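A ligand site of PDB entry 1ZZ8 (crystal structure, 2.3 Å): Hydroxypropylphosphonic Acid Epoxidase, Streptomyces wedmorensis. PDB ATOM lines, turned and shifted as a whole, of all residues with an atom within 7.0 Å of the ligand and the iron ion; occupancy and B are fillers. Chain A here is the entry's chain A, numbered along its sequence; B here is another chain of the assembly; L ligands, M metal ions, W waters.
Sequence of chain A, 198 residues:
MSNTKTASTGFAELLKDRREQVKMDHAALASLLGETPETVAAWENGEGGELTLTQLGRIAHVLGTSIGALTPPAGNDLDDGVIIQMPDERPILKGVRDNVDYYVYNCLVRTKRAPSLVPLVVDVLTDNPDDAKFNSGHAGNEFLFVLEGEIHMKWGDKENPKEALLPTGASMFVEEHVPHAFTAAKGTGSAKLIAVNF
NH2 of Arg 97 is in salt-bridge range of O2 of the ligand (2.6 Å).
The side-chain amino group (NZ) of Lys 23 of chain B is in salt-bridge range of an oxygen (O4) of the ligand, at 3.7 Å.
ND2 of Asn 135 lies within hydrogen-bond range of O2 of the ligand (3.0 Å).
An oxygen (O4) of the ligand lies within hydrogen-bond range of the side-chain hydroxyl (OH) of Tyr 105 (2.8 Å).
The guanidinium group of Arg 97 sits at hydrogen-bond distance from the backbone carbonyl oxygen of Lys 133 (3.0 Å).
ND1 of His 180 sits at hydrogen-bond distance from O of Val 178 (2.7 Å).
N of Gly 137 sits at hydrogen-bond distance from OD1 of Asn 135, at 2.8 Å.
The side-chain carboxylate of Glu 142 sits close to the side-chain amide oxygen of Asn 197 (3.3 Å).
The backbone NH (N) of His 180 lies within hydrogen-bond range of the side-chain amide oxygen (OD1) of Asn 135, at 3.1 Å.
The side-chain amino group of Lys 23 of chain B is in hydrogen-bond range of the backbone carbonyl oxygen of Glu 20 of chain B (3.3 Å).
The backbone carbonyl oxygen (O) of Phe 182 sits at hydrogen-bond distance from the side-chain hydroxyl (OH) of Tyr 102 (2.8 Å).
The backbone NH (N) of Val 174 sits at hydrogen-bond distance from the backbone carbonyl oxygen (O) of Glu 142 (3.0 Å).
Tyr 103 touches the ligand (CE2 to O2, 3.7 Å).
CD1 of Phe 182 touches C3 of the ligand (3.9 Å).
Hydrophobic or aromatic side chains within 4 Å of the ligand: Tyr 103, Tyr 105, His 138, His 180 and Phe 182.
Of the 24 residues printed, 9 come within 4 Å of the ligand.
Within 4 Å of the iron ion: His 138, Glu 142 and His 180.
The nearest printed residue that does not touch the iron ion is Asn 135 (4.1 Å).
The iron ion is bound by an oxygen (O3) of the ligand, the side-chain carboxylate (OE2) of Glu 142, a ring nitrogen (NE2) of His 138, a ring nitrogen (NE2) of His 180 and an oxygen (O1) of the ligand.
Water W1 lies within hydrogen-bond range of the side-chain amino group (NZ) of Lys 23 of chain B (2.5 Å) and an oxygen (O4) of the ligand (3.0 Å).
Water W2 lies within hydrogen-bond range of an oxygen (O2) of the ligand (2.7 Å), the side-chain hydroxyl of Tyr 103 (2.7 Å), the guanidinium group of Arg 97 (2.9 Å), the backbone carbonyl oxygen of His 180 (3.0 Å) and the side-chain amide nitrogen of Asn 135 (3.4 Å).
Water W3 lies within hydrogen-bond range of the side-chain carboxylate of Glu 142 (2.7 Å) and the side-chain amide oxygen of Asn 197 (3.1 Å).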
ATOM      1  N   ARG A  97      27.141 -14.887 -15.603  1.00  0.00           N
ATOM      2  CA  ARG A  97      26.496 -14.491 -16.848  1.00  0.00           C
ATOM      3  C   ARG A  97      27.478 -14.678 -17.981  1.00  0.00           C
ATOM      4  O   ARG A  97      28.591 -14.132 -17.935  1.00  0.00           O
ATOM      5  CB  ARG A  97      26.036 -13.034 -16.819  1.00  0.00           C
ATOM      6  CG  ARG A  97      24.992 -12.781 -15.789  1.00  0.00           C
ATOM      7  CD  ARG A  97      24.271 -11.466 -15.992  1.00  0.00           C
ATOM      8  NE  ARG A  97      23.259 -11.344 -14.960  1.00  0.00           N
ATOM      9  CZ  ARG A  97      22.533 -10.262 -14.725  1.00  0.00           C
ATOM     10  NH1 ARG A  97      22.690  -9.160 -15.461  1.00  0.00           N
ATOM     11  NH2 ARG A  97      21.645 -10.288 -13.735  1.00  0.00           N
ATOM     12  N   TYR A 102      29.669 -12.674 -12.152  1.00  0.00           N
ATOM     13  CA  TYR A 102      29.259 -11.290 -12.330  1.00  0.00           C
ATOM     14  C   TYR A 102      28.787 -10.634 -11.036  1.00  0.00           C
ATOM     15  O   TYR A 102      29.155  -9.508 -10.737  1.00  0.00           O
ATOM     16  CB  TYR A 102      28.157 -11.247 -13.383  1.00  0.00           C
ATOM     17  CG  TYR A 102      28.035  -9.919 -14.069  1.00  0.00           C
ATOM     18  CD1 TYR A 102      28.965  -9.528 -15.042  1.00  0.00           C
ATOM     19  CD2 TYR A 102      27.010  -9.042 -13.736  1.00  0.00           C
ATOM     20  CE1 TYR A 102      28.865  -8.288 -15.654  1.00  0.00           C
ATOM     21  CE2 TYR A 102      26.909  -7.808 -14.342  1.00  0.00           C
ATOM     22  CZ  TYR A 102      27.827  -7.433 -15.304  1.00  0.00           C
ATOM     23  OH  TYR A 102      27.715  -6.208 -15.906  1.00  0.00           O
ATOM     24  N   TYR A 103      27.941 -11.344 -10.283  1.00  0.00           N
ATOM     25  CA  TYR A 103      27.421 -10.861  -9.015  1.00  0.00           C
ATOM     26  C   TYR A 103      27.459 -12.017  -8.041  1.00  0.00           C
ATOM     27  O   TYR A 103      27.608 -13.177  -8.427  1.00  0.00           O
ATOM     28  CB  TYR A 103      25.939 -10.454  -9.094  1.00  0.00           C
ATOM     29  CG  TYR A 103      25.537  -9.403 -10.080  1.00  0.00           C
ATOM     30  CD1 TYR A 103      26.276  -8.225 -10.207  1.00  0.00           C
ATOM     31  CD2 TYR A 103      24.387  -9.556 -10.866  1.00  0.00           C
ATOM     32  CE1 TYR A 103      25.879  -7.226 -11.087  1.00  0.00           C
ATOM     33  CE2 TYR A 103      23.967  -8.553 -11.746  1.00  0.00           C
ATOM     34  CZ  TYR A 103      24.731  -7.392 -11.843  1.00  0.00           C
ATOM     35  OH  TYR A 103      24.355  -6.374 -12.700  1.00  0.00           O
ATOM     36  N   TYR A 105      24.946 -12.941  -4.765  1.00  0.00           N
ATOM     37  CA  TYR A 105      23.731 -12.444  -4.134  1.00  0.00           C
ATOM     38  C   TYR A 105      23.642 -12.812  -2.659  1.00  0.00           C
ATOM     39  O   TYR A 105      23.548 -13.992  -2.321  1.00  0.00           O
ATOM     40  CB  TYR A 105      22.474 -12.975  -4.833  1.00  0.00           C
ATOM     41  CG  TYR A 105      22.309 -12.579  -6.266  1.00  0.00           C
ATOM     42  CD1 TYR A 105      22.622 -13.469  -7.296  1.00  0.00           C
ATOM     43  CD2 TYR A 105      21.827 -11.320  -6.613  1.00  0.00           C
ATOM     44  CE1 TYR A 105      22.433 -13.109  -8.641  1.00  0.00           C
ATOM     45  CE2 TYR A 105      21.631 -10.946  -7.945  1.00  0.00           C
ATOM     46  CZ  TYR A 105      21.950 -11.856  -8.950  1.00  0.00           C
ATOM     47  OH  TYR A 105      21.804 -11.481 -10.272  1.00  0.00           O
ATOM     48  N   LEU A 120      18.355  -7.432  -1.183  1.00  0.00           N
ATOM     49  CA  LEU A 120      19.653  -8.081  -1.295  1.00  0.00           C
ATOM     50  C   LEU A 120      20.862  -7.149  -1.243  1.00  0.00           C
ATOM     51  O   LEU A 120      20.772  -5.958  -1.546  1.00  0.00           O
ATOM     52  CB  LEU A 120      19.759  -8.801  -2.646  1.00  0.00           C
ATOM     53  CG  LEU A 120      18.618  -9.569  -3.293  1.00  0.00           C
ATOM     54  CD1 LEU A 120      18.848  -9.591  -4.806  1.00  0.00           C
ATOM     55  CD2 LEU A 120      18.548 -10.980  -2.725  1.00  0.00           C
ATOM     56  N   VAL A 122      24.138  -6.940  -3.118  1.00  0.00           N
ATOM     57  CA  VAL A 122      24.726  -7.504  -4.328  1.00  0.00           C
ATOM     58  C   VAL A 122      26.162  -7.033  -4.501  1.00  0.00           C
ATOM     59  O   VAL A 122      26.417  -5.824  -4.539  1.00  0.00           O
ATOM     60  CB  VAL A 122      23.934  -7.087  -5.592  1.00  0.00           C
ATOM     61  CG1 VAL A 122      24.540  -7.734  -6.812  1.00  0.00           C
ATOM     62  CG2 VAL A 122      22.458  -7.450  -5.446  1.00  0.00           C
ATOM     63  N   VAL A 124      29.042  -6.337  -6.828  1.00  0.00           N
ATOM     64  CA  VAL A 124      29.321  -6.154  -8.239  1.00  0.00           C
ATOM     65  C   VAL A 124      30.785  -6.581  -8.412  1.00  0.00           C
ATOM     66  O   VAL A 124      31.697  -5.844  -8.052  1.00  0.00           O
ATOM     67  CB  VAL A 124      29.116  -4.685  -8.654  1.00  0.00           C
ATOM     68  CG1 VAL A 124      29.392  -4.519 -10.142  1.00  0.00           C
ATOM     69  CG2 VAL A 124      27.696  -4.244  -8.302  1.00  0.00           C
ATOM     70  N   LYS A 133      27.436  -6.963 -18.463  1.00  0.00           N
ATOM     71  CA  LYS A 133      26.492  -7.959 -18.919  1.00  0.00           C
ATOM     72  C   LYS A 133      25.051  -7.739 -18.464  1.00  0.00           C
ATOM     73  O   LYS A 133      24.710  -7.855 -17.281  1.00  0.00           O
ATOM     74  CB  LYS A 133      26.999  -9.358 -18.580  1.00  0.00           C
ATOM     75  CG  LYS A 133      27.991  -9.799 -19.652  1.00  0.00           C
ATOM     76  CD  LYS A 133      28.916 -10.919 -19.259  1.00  0.00           C
ATOM     77  CE  LYS A 133      30.011 -11.029 -20.323  1.00  0.00           C
ATOM     78  NZ  LYS A 133      31.035 -12.075 -20.038  1.00  0.00           N
ATOM     79  N   PHE A 134      24.229  -7.394 -19.449  1.00  0.00           N
ATOM     80  CA  PHE A 134      22.812  -7.116 -19.247  1.00  0.00           C
ATOM     81  C   PHE A 134      21.960  -8.315 -18.874  1.00  0.00           C
ATOM     82  O   PHE A 134      22.366  -9.464 -19.045  1.00  0.00           O
ATOM     83  CB  PHE A 134      22.213  -6.528 -20.534  1.00  0.00           C
ATOM     84  CG  PHE A 134      22.272  -5.041 -20.598  1.00  0.00           C
ATOM     85  CD1 PHE A 134      23.500  -4.382 -20.661  1.00  0.00           C
ATOM     86  CD2 PHE A 134      21.110  -4.289 -20.559  1.00  0.00           C
ATOM     87  CE1 PHE A 134      23.562  -3.008 -20.681  1.00  0.00           C
ATOM     88  CE2 PHE A 134      21.157  -2.916 -20.568  1.00  0.00           C
ATOM     89  CZ  PHE A 134      22.386  -2.257 -20.631  1.00  0.00           C
ATOM     90  N   ASN A 135      20.803  -8.034 -18.307  1.00  0.00           N
ATOM     91  CA  ASN A 135      19.833  -9.082 -18.033  1.00  0.00           C
ATOM     92  C   ASN A 135      18.773  -8.645 -19.053  1.00  0.00           C
ATOM     93  O   ASN A 135      19.052  -7.772 -19.883  1.00  0.00           O
ATOM     94  CB  ASN A 135      19.305  -9.051 -16.591  1.00  0.00           C
ATOM     95  CG  ASN A 135      18.663  -7.728 -16.215  1.00  0.00           C
ATOM     96  OD1 ASN A 135      18.090  -7.033 -17.060  1.00  0.00           O
ATOM     97  ND2 ASN A 135      18.739  -7.392 -14.932  1.00  0.00           N
ATOM     98  N   GLY A 137      15.590  -7.440 -18.283  1.00  0.00           N
ATOM     99  CA  GLY A 137      14.485  -6.865 -17.540  1.00  0.00           C
ATOM    100  C   GLY A 137      13.858  -7.954 -16.716  1.00  0.00           C
ATOM    101  O   GLY A 137      14.078  -9.148 -16.981  1.00  0.00           O
ATOM    102  N   HIS A 138      13.088  -7.568 -15.704  1.00  0.00           N
ATOM    103  CA  HIS A 138      12.415  -8.513 -14.844  1.00  0.00           C
ATOM    104  C   HIS A 138      11.172  -7.871 -14.228  1.00  0.00           C
ATOM    105  O   HIS A 138      11.102  -6.644 -14.077  1.00  0.00           O
ATOM    106  CB  HIS A 138      13.357  -9.050 -13.745  1.00  0.00           C
ATOM    107  CG  HIS A 138      13.957  -7.981 -12.876  1.00  0.00           C
ATOM    108  ND1 HIS A 138      13.208  -7.062 -12.180  1.00  0.00           N
ATOM    109  CD2 HIS A 138      15.248  -7.719 -12.556  1.00  0.00           C
ATOM    110  CE1 HIS A 138      14.006  -6.278 -11.478  1.00  0.00           C
ATOM    111  NE2 HIS A 138      15.251  -6.660 -11.687  1.00  0.00           N
ATOM    112  N   GLU A 142      12.536  -1.979  -8.831  1.00  0.00           N
ATOM    113  CA  GLU A 142      13.697  -2.209  -7.985  1.00  0.00           C
ATOM    114  C   GLU A 142      14.364  -0.930  -7.479  1.00  0.00           C
ATOM    115  O   GLU A 142      14.717  -0.029  -8.254  1.00  0.00           O
ATOM    116  CB  GLU A 142      14.713  -3.076  -8.738  1.00  0.00           C
ATOM    117  CG  GLU A 142      15.917  -3.471  -7.909  1.00  0.00           C
ATOM    118  CD  GLU A 142      16.939  -4.311  -8.690  1.00  0.00           C
ATOM    119  OE1 GLU A 142      18.035  -4.562  -8.149  1.00  0.00           O
ATOM    120  OE2 GLU A 142      16.637  -4.718  -9.841  1.00  0.00           O
ATOM    121  N   LEU A 144      17.621   0.748  -5.570  1.00  0.00           N
ATOM    122  CA  LEU A 144      19.033   0.437  -5.363  1.00  0.00           C
ATOM    123  C   LEU A 144      19.788   1.544  -4.657  1.00  0.00           C
ATOM    124  O   LEU A 144      19.489   2.731  -4.815  1.00  0.00           O
ATOM    125  CB  LEU A 144      19.721   0.105  -6.693  1.00  0.00           C
ATOM    126  CG  LEU A 144      19.277  -1.218  -7.333  1.00  0.00           C
ATOM    127  CD1 LEU A 144      18.304  -0.901  -8.458  1.00  0.00           C
ATOM    128  CD2 LEU A 144      20.480  -1.984  -7.866  1.00  0.00           C
ATOM    129  N   VAL A 174      14.604   1.524 -10.772  1.00  0.00           N
ATOM    130  CA  VAL A 174      14.534   0.880 -12.079  1.00  0.00           C
ATOM    131  C   VAL A 174      13.154   0.247 -12.245  1.00  0.00           C
ATOM    132  O   VAL A 174      12.833  -0.755 -11.609  1.00  0.00           O
ATOM    133  CB  VAL A 174      15.587  -0.222 -12.232  1.00  0.00           C
ATOM    134  CG1 VAL A 174      15.473  -0.853 -13.605  1.00  0.00           C
ATOM    135  CG2 VAL A 174      16.983   0.346 -11.986  1.00  0.00           C
ATOM    136  N   VAL A 178      12.486  -3.015 -17.458  1.00  0.00           N
ATOM    137  CA  VAL A 178      13.627  -2.281 -17.991  1.00  0.00           C
ATOM    138  C   VAL A 178      14.913  -3.104 -17.764  1.00  0.00           C
ATOM    139  O   VAL A 178      15.301  -3.364 -16.612  1.00  0.00           O
ATOM    140  CB  VAL A 178      13.786  -0.927 -17.283  1.00  0.00           C
ATOM    141  CG1 VAL A 178      14.993  -0.183 -17.823  1.00  0.00           C
ATOM    142  CG2 VAL A 178      12.504  -0.108 -17.455  1.00  0.00           C
ATOM    143  N   HIS A 180      18.844  -4.015 -17.389  1.00  0.00           N
ATOM    144  CA  HIS A 180      19.933  -3.229 -16.819  1.00  0.00           C
ATOM    145  C   HIS A 180      21.156  -4.079 -16.488  1.00  0.00           C
ATOM    146  O   HIS A 180      21.065  -5.313 -16.418  1.00  0.00           O
ATOM    147  CB  HIS A 180      19.430  -2.522 -15.550  1.00  0.00           C
ATOM    148  CG  HIS A 180      18.638  -3.418 -14.647  1.00  0.00           C
ATOM    149  ND1 HIS A 180      17.325  -3.752 -14.900  1.00  0.00           N
ATOM    150  CD2 HIS A 180      18.976  -4.087 -13.530  1.00  0.00           C
ATOM    151  CE1 HIS A 180      16.895  -4.600 -13.986  1.00  0.00           C
ATOM    152  NE2 HIS A 180      17.880  -4.820 -13.132  1.00  0.00           N
ATOM    153  N   ALA A 181      22.270  -3.403 -16.254  1.00  0.00           N
ATOM    154  CA  ALA A 181      23.534  -4.039 -15.928  1.00  0.00           C
ATOM    155  C   ALA A 181      24.411  -3.123 -15.078  1.00  0.00           C
ATOM    156  O   ALA A 181      24.350  -1.899 -15.200  1.00  0.00           O
ATOM    157  CB  ALA A 181      24.263  -4.399 -17.208  1.00  0.00           C
ATOM    158  N   PHE A 182      25.225  -3.717 -14.203  1.00  0.00           N
ATOM    159  CA  PHE A 182      26.121  -2.947 -13.341  1.00  0.00           C
ATOM    160  C   PHE A 182      27.523  -3.547 -13.312  1.00  0.00           C
ATOM    161  O   PHE A 182      27.715  -4.749 -13.489  1.00  0.00           O
ATOM    162  CB  PHE A 182      25.606  -2.871 -11.894  1.00  0.00           C
ATOM    163  CG  PHE A 182      24.237  -2.266 -11.740  1.00  0.00           C
ATOM    164  CD1 PHE A 182      23.104  -3.052 -11.802  1.00  0.00           C
ATOM    165  CD2 PHE A 182      24.092  -0.905 -11.523  1.00  0.00           C
ATOM    166  CE1 PHE A 182      21.839  -2.504 -11.644  1.00  0.00           C
ATOM    167  CE2 PHE A 182      22.836  -0.334 -11.369  1.00  0.00           C
ATOM    168  CZ  PHE A 182      21.703  -1.141 -11.424  1.00  0.00           C
ATOM    169  N   LEU A 193      26.127  -3.025  -3.641  1.00  0.00           N
ATOM    170  CA  LEU A 193      24.867  -2.316  -3.606  1.00  0.00           C
ATOM    171  C   LEU A 193      23.751  -3.091  -2.938  1.00  0.00           C
ATOM    172  O   LEU A 193      23.774  -4.324  -2.889  1.00  0.00           O
ATOM    173  CB  LEU A 193      24.445  -1.916  -5.037  1.00  0.00           C
ATOM    174  CG  LEU A 193      24.313  -2.982  -6.122  1.00  0.00           C
ATOM    175  CD1 LEU A 193      23.241  -3.990  -5.725  1.00  0.00           C
ATOM    176  CD2 LEU A 193      23.938  -2.342  -7.460  1.00  0.00           C
ATOM    177  N   ALA A 195      19.953  -4.073  -3.181  1.00  0.00           N
ATOM    178  CA  ALA A 195      18.894  -4.092  -4.174  1.00  0.00           C
ATOM    179  C   ALA A 195      17.594  -4.596  -3.566  1.00  0.00           C
ATOM    180  O   ALA A 195      17.535  -5.705  -3.021  1.00  0.00           O
ATOM    181  CB  ALA A 195      19.316  -4.979  -5.338  1.00  0.00           C
ATOM    182  N   ASN A 197      13.789  -5.478  -4.496  1.00  0.00           N
ATOM    183  CA  ASN A 197      12.762  -5.729  -5.503  1.00  0.00           C
ATOM    184  C   ASN A 197      11.475  -5.801  -4.701  1.00  0.00           C
ATOM    185  O   ASN A 197      11.423  -6.489  -3.686  1.00  0.00           O
ATOM    186  CB  ASN A 197      13.008  -7.053  -6.223  1.00  0.00           C
ATOM    187  CG  ASN A 197      14.378  -7.106  -6.895  1.00  0.00           C
ATOM    188  OD1 ASN A 197      14.616  -6.441  -7.913  1.00  0.00           O
ATOM    189  ND2 ASN A 197      15.294  -7.891  -6.323  1.00  0.00           N
ATOM    190  N   GLU B  20      14.009 -17.822  -9.870  1.00  0.00           N
ATOM    191  CA  GLU B  20      14.969 -16.810 -10.283  1.00  0.00           C
ATOM    192  C   GLU B  20      14.799 -15.461  -9.581  1.00  0.00           C
ATOM    193  O   GLU B  20      15.785 -14.741  -9.368  1.00  0.00           O
ATOM    194  CB  GLU B  20      14.909 -16.617 -11.802  1.00  0.00           C
ATOM    195  CG  GLU B  20      15.429 -17.825 -12.600  1.00  0.00           C
ATOM    196  CD  GLU B  20      15.447 -17.605 -14.107  1.00  0.00           C
ATOM    197  OE1 GLU B  20      16.188 -18.340 -14.804  1.00  0.00           O
ATOM    198  OE2 GLU B  20      14.719 -16.710 -14.592  1.00  0.00           O
ATOM    199  N   LYS B  23      16.562 -15.680  -6.142  1.00  0.00           N
ATOM    200  CA  LYS B  23      17.960 -16.068  -6.173  1.00  0.00           C
ATOM    201  C   LYS B  23      18.306 -17.454  -5.650  1.00  0.00           C
ATOM    202  O   LYS B  23      19.045 -17.605  -4.669  1.00  0.00           O
ATOM    203  CB  LYS B  23      18.790 -15.027  -5.434  1.00  0.00           C
ATOM    204  CG  LYS B  23      19.149 -13.836  -6.303  1.00  0.00           C
ATOM    205  CD  LYS B  23      17.918 -13.236  -6.930  1.00  0.00           C
ATOM    206  CE  LYS B  23      18.308 -12.278  -7.999  1.00  0.00           C
ATOM    207  NZ  LYS B  23      17.105 -11.777  -8.693  1.00  0.00           N
HETATM  208  P1  LIG L   1      19.708  -8.580 -11.307  1.00  0.00           P
HETATM  209  C1  LIG L   1      20.494  -7.747  -9.899  1.00  0.00           C
HETATM  210  C2  LIG L   1      20.825  -6.304 -10.274  1.00  0.00           C
HETATM  211  O1  LIG L   1      19.731  -5.481  -9.995  1.00  0.00           O
HETATM  212  C3  LIG L   1      21.652  -5.947  -9.640  1.00  0.00           C
HETATM  213  O2  LIG L   1      20.391  -8.373 -12.567  1.00  0.00           O
HETATM  214  O3  LIG L   1      18.222  -8.095 -11.380  1.00  0.00           O
HETATM  215  O4  LIG L   1      19.467 -10.075 -10.954  1.00  0.00           O
HETATM  216 FE    FE M   1      17.516  -6.159 -11.169  1.00  0.00          FE
HETATM  217  O   HOH W   1      16.577  -9.762 -10.146  1.00  0.00           O
HETATM  218  O   HOH W   2      21.985  -6.763 -13.969  1.00  0.00           O
HETATM  219  O   HOH W   3      17.603  -7.263  -8.417  1.00  0.00           O
